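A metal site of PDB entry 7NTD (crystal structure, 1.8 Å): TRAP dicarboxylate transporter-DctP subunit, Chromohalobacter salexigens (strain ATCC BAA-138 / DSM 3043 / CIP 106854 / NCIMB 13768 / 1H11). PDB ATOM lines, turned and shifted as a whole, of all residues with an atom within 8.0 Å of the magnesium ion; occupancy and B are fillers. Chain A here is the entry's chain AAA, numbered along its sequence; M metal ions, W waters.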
ATOM      1  N   ASP A  59     -17.141 -18.683  -3.277  1.00  0.00           N
ATOM      2  CA  ASP A  59     -17.880 -19.790  -2.593  1.00  0.00           C
ATOM      3  C   ASP A  59     -19.377 -19.480  -2.546  1.00  0.00           C
ATOM      4  O   ASP A  59     -20.186 -20.440  -2.599  1.00  0.00           O
ATOM      5  CB  ASP A  59     -17.286 -20.100  -1.230  1.00  0.00           C
ATOM      6  CG  ASP A  59     -16.026 -20.934  -1.365  1.00  0.00           C
ATOM      7  OD1 ASP A  59     -15.947 -21.709  -2.338  1.00  0.00           O
ATOM      8  OD2 ASP A  59     -15.118 -20.774  -0.530  1.00  0.00           O
ATOM      9  N   GLN A  60     -19.763 -18.190  -2.482  1.00  0.00           N
ATOM     10  CA  GLN A  60     -21.195 -17.815  -2.482  1.00  0.00           C
ATOM     11  C   GLN A  60     -21.858 -18.392  -3.735  1.00  0.00           C
ATOM     12  O   GLN A  60     -23.008 -18.815  -3.646  1.00  0.00           O
ATOM     13  CB  GLN A  60     -21.433 -16.303  -2.390  1.00  0.00           C
ATOM     14  CG  GLN A  60     -21.032 -15.693  -1.047  1.00  0.00           C
ATOM     15  CD  GLN A  60     -21.557 -14.292  -0.827  1.00  0.00           C
ATOM     16  OE1 GLN A  60     -22.529 -13.861  -1.436  1.00  0.00           O
ATOM     17  NE2 GLN A  60     -20.945 -13.607   0.120  1.00  0.00           N
ATOM     18  N   ALA A  61     -21.177 -18.380  -4.882  1.00  0.00           N
ATOM     19  CA  ALA A  61     -21.709 -18.934  -6.163  1.00  0.00           C
ATOM     20  C   ALA A  61     -21.579 -20.457  -6.136  1.00  0.00           C
ATOM     21  O   ALA A  61     -22.573 -21.139  -6.347  1.00  0.00           O
ATOM     22  CB  ALA A  61     -20.984 -18.368  -7.350  1.00  0.00           C
ATOM     23  N   LYS A  62     -20.383 -20.964  -5.857  1.00  0.00           N
ATOM     24  CA  LYS A  62     -20.083 -22.403  -5.910  1.00  0.00           C
ATOM     25  C   LYS A  62     -21.080 -23.159  -5.011  1.00  0.00           C
ATOM     26  O   LYS A  62     -21.451 -24.268  -5.392  1.00  0.00           O
ATOM     27  CB  LYS A  62     -18.654 -22.699  -5.469  1.00  0.00           C
ATOM     28  CG  LYS A  62     -18.234 -24.154  -5.565  1.00  0.00           C
ATOM     29  CD  LYS A  62     -16.749 -24.374  -5.464  1.00  0.00           C
ATOM     30  CE  LYS A  62     -16.376 -25.816  -5.187  1.00  0.00           C
ATOM     31  NZ  LYS A  62     -14.917 -26.032  -5.304  1.00  0.00           N
ATOM     32  N   ASP A  63     -21.481 -22.569  -3.878  1.00  0.00           N
ATOM     33  CA  ASP A  63     -22.301 -23.221  -2.817  1.00  0.00           C
ATOM     34  C   ASP A  63     -23.776 -22.795  -2.897  1.00  0.00           C
ATOM     35  O   ASP A  63     -24.555 -23.225  -2.031  1.00  0.00           O
ATOM     36  CB  ASP A  63     -21.715 -22.909  -1.434  1.00  0.00           C
ATOM     37  CG  ASP A  63     -20.295 -23.428  -1.261  1.00  0.00           C
ATOM     38  OD1 ASP A  63     -19.851 -24.208  -2.117  1.00  0.00           O
ATOM     39  OD2 ASP A  63     -19.644 -23.039  -0.286  1.00  0.00           O
ATOM     40  N   GLY A  64     -24.154 -21.955  -3.859  1.00  0.00           N
ATOM     41  CA  GLY A  64     -25.567 -21.650  -4.157  1.00  0.00           C
ATOM     42  C   GLY A  64     -26.222 -20.674  -3.198  1.00  0.00           C
ATOM     43  O   GLY A  64     -27.456 -20.615  -3.203  1.00  0.00           O
ATOM     44  N   GLN A  65     -25.453 -19.870  -2.446  1.00  0.00           N
ATOM     45  CA  GLN A  65     -26.024 -18.771  -1.622  1.00  0.00           C
ATOM     46  C   GLN A  65     -26.525 -17.676  -2.572  1.00  0.00           C
ATOM     47  O   GLN A  65     -27.549 -17.058  -2.287  1.00  0.00           O
ATOM     48  CB  GLN A  65     -24.993 -18.229  -0.626  1.00  0.00           C
ATOM     49  CG  GLN A  65     -24.258 -19.341   0.126  1.00  0.00           C
ATOM     50  CD  GLN A  65     -23.702 -18.883   1.453  1.00  0.00           C
ATOM     51  OE1 GLN A  65     -24.401 -18.293   2.268  1.00  0.00           O
ATOM     52  NE2 GLN A  65     -22.439 -19.192   1.685  1.00  0.00           N
ATOM     53  N   VAL A  66     -25.786 -17.434  -3.660  1.00  0.00           N
ATOM     54  CA  VAL A  66     -26.197 -16.577  -4.807  1.00  0.00           C
ATOM     55  C   VAL A  66     -25.988 -17.404  -6.080  1.00  0.00           C
ATOM     56  O   VAL A  66     -25.410 -18.521  -5.989  1.00  0.00           O
ATOM     57  CB  VAL A  66     -25.459 -15.218  -4.798  1.00  0.00           C
ATOM     58  CG1 VAL A  66     -25.630 -14.492  -3.478  1.00  0.00           C
ATOM     59  CG2 VAL A  66     -23.989 -15.349  -5.162  1.00  0.00           C
ATOM     60  N   GLY A 116     -17.143 -26.684 -10.311  1.00  0.00           N
ATOM     61  CA  GLY A 116     -18.203 -26.228  -9.386  1.00  0.00           C
ATOM     62  C   GLY A 116     -18.752 -24.862  -9.765  1.00  0.00           C
ATOM     63  O   GLY A 116     -19.782 -24.445  -9.210  1.00  0.00           O
ATOM     64  N   VAL A 117     -18.144 -24.194 -10.759  1.00  0.00           N
ATOM     65  CA  VAL A 117     -18.777 -22.989 -11.366  1.00  0.00           C
ATOM     66  C   VAL A 117     -18.800 -23.148 -12.885  1.00  0.00           C
ATOM     67  O   VAL A 117     -17.926 -23.804 -13.447  1.00  0.00           O
ATOM     68  CB  VAL A 117     -18.129 -21.657 -10.910  1.00  0.00           C
ATOM     69  CG1 VAL A 117     -18.021 -21.609  -9.390  1.00  0.00           C
ATOM     70  CG2 VAL A 117     -16.789 -21.407 -11.565  1.00  0.00           C
ATOM     71  N   MET A 223     -21.054 -18.577 -12.397  1.00  0.00           N
ATOM     72  CA  MET A 223     -22.429 -18.962 -11.997  1.00  0.00           C
ATOM     73  C   MET A 223     -22.328 -20.298 -11.272  1.00  0.00           C
ATOM     74  O   MET A 223     -21.440 -21.048 -11.632  1.00  0.00           O
ATOM     75  CB  MET A 223     -23.314 -19.105 -13.236  1.00  0.00           C
ATOM     76  CG  MET A 223     -24.717 -19.604 -12.962  1.00  0.00           C
ATOM     77  SD  MET A 223     -25.607 -19.597 -14.533  1.00  0.00           S
ATOM     78  CE  MET A 223     -27.303 -19.659 -13.963  1.00  0.00           C
ATOM     79  N   ASP A 224     -23.175 -20.542 -10.279  1.00  0.00           N
ATOM     80  CA  ASP A 224     -23.225 -21.826  -9.531  1.00  0.00           C
ATOM     81  C   ASP A 224     -23.508 -22.921 -10.565  1.00  0.00           C
ATOM     82  O   ASP A 224     -24.496 -22.767 -11.280  1.00  0.00           O
ATOM     83  CB  ASP A 224     -24.323 -21.772  -8.465  1.00  0.00           C
ATOM     84  CG  ASP A 224     -24.560 -23.041  -7.670  1.00  0.00           C
ATOM     85  OD1 ASP A 224     -23.709 -23.970  -7.746  1.00  0.00           O
ATOM     86  OD2 ASP A 224     -25.584 -23.081  -6.983  1.00  0.00           O
ATOM     87  N   GLN A 225     -22.646 -23.919 -10.671  1.00  0.00           N
ATOM     88  CA  GLN A 225     -22.812 -25.010 -11.678  1.00  0.00           C
ATOM     89  C   GLN A 225     -24.150 -25.725 -11.462  1.00  0.00           C
ATOM     90  O   GLN A 225     -24.721 -26.249 -12.456  1.00  0.00           O
ATOM     91  CB  GLN A 225     -21.646 -25.992 -11.598  1.00  0.00           C
ATOM     92  CG  GLN A 225     -21.635 -27.034 -12.708  1.00  0.00           C
ATOM     93  CD  GLN A 225     -21.516 -26.394 -14.063  1.00  0.00           C
ATOM     94  OE1 GLN A 225     -20.521 -25.741 -14.384  1.00  0.00           O
ATOM     95  NE2 GLN A 225     -22.541 -26.566 -14.885  1.00  0.00           N
ATOM     96  N   ASP A 226     -24.633 -25.758 -10.215  1.00  0.00           N
ATOM     97  CA  ASP A 226     -25.924 -26.371  -9.802  1.00  0.00           C
ATOM     98  C   ASP A 226     -27.098 -25.530 -10.326  1.00  0.00           C
ATOM     99  O   ASP A 226     -28.113 -26.135 -10.670  1.00  0.00           O
ATOM    100  CB  ASP A 226     -26.017 -26.558  -8.284  1.00  0.00           C
ATOM    101  CG  ASP A 226     -24.933 -27.463  -7.740  1.00  0.00           C
ATOM    102  OD1 ASP A 226     -25.165 -28.678  -7.671  1.00  0.00           O
ATOM    103  OD2 ASP A 226     -23.834 -26.962  -7.436  1.00  0.00           O
ATOM    104  N   LYS A 227     -26.988 -24.198 -10.377  1.00  0.00           N
ATOM    105  CA  LYS A 227     -28.128 -23.343 -10.831  1.00  0.00           C
ATOM    106  C   LYS A 227     -28.254 -23.497 -12.346  1.00  0.00           C
ATOM    107  O   LYS A 227     -29.398 -23.686 -12.834  1.00  0.00           O
ATOM    108  CB  LYS A 227     -27.953 -21.879 -10.443  1.00  0.00           C
ATOM    109  CG  LYS A 227     -29.184 -21.019 -10.676  1.00  0.00           C
ATOM    110  CD  LYS A 227     -30.407 -21.475  -9.915  1.00  0.00           C
ATOM    111  CE  LYS A 227     -31.595 -20.555 -10.105  1.00  0.00           C
ATOM    112  NZ  LYS A 227     -32.447 -20.498  -8.902  1.00  0.00           N
HETATM  113 MG    MG M   1     -23.048 -25.434  -6.290  1.00  0.00          MG
HETATM  114  O   HOH W   1     -22.428 -26.724  -5.030  1.00  0.00           O
HETATM  115  O   HOH W   2     -24.542 -25.029  -5.225  1.00  0.00           O
HETATM  116  O   HOH W   3     -21.411 -25.922  -7.451  1.00  0.00           O
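The magnesium ion is bound by water W2 (1.9 Å), water W1 (1.9 Å), water W3 (2.1 Å), the side-chain carboxylate (OD2) of Asp 226 (2.1 Å), the side-chain carboxylate (OD1) of Asp 224 (2.2 Å) and the backbone carbonyl oxygen (O) of Lys 62 (2.2 Å).
Water W2 lies within hydrogen-bond range of OD2 of Asp 224 (2.8 Å) and N of Gly 64 (3.4 Å).
Three residues have an atom within 4 Å of the magnesium ion: Lys 62, Asp 224 and Asp 226.
The nearest printed residue that does not touch the magnesium ion is Asp 63 (4.1 Å).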
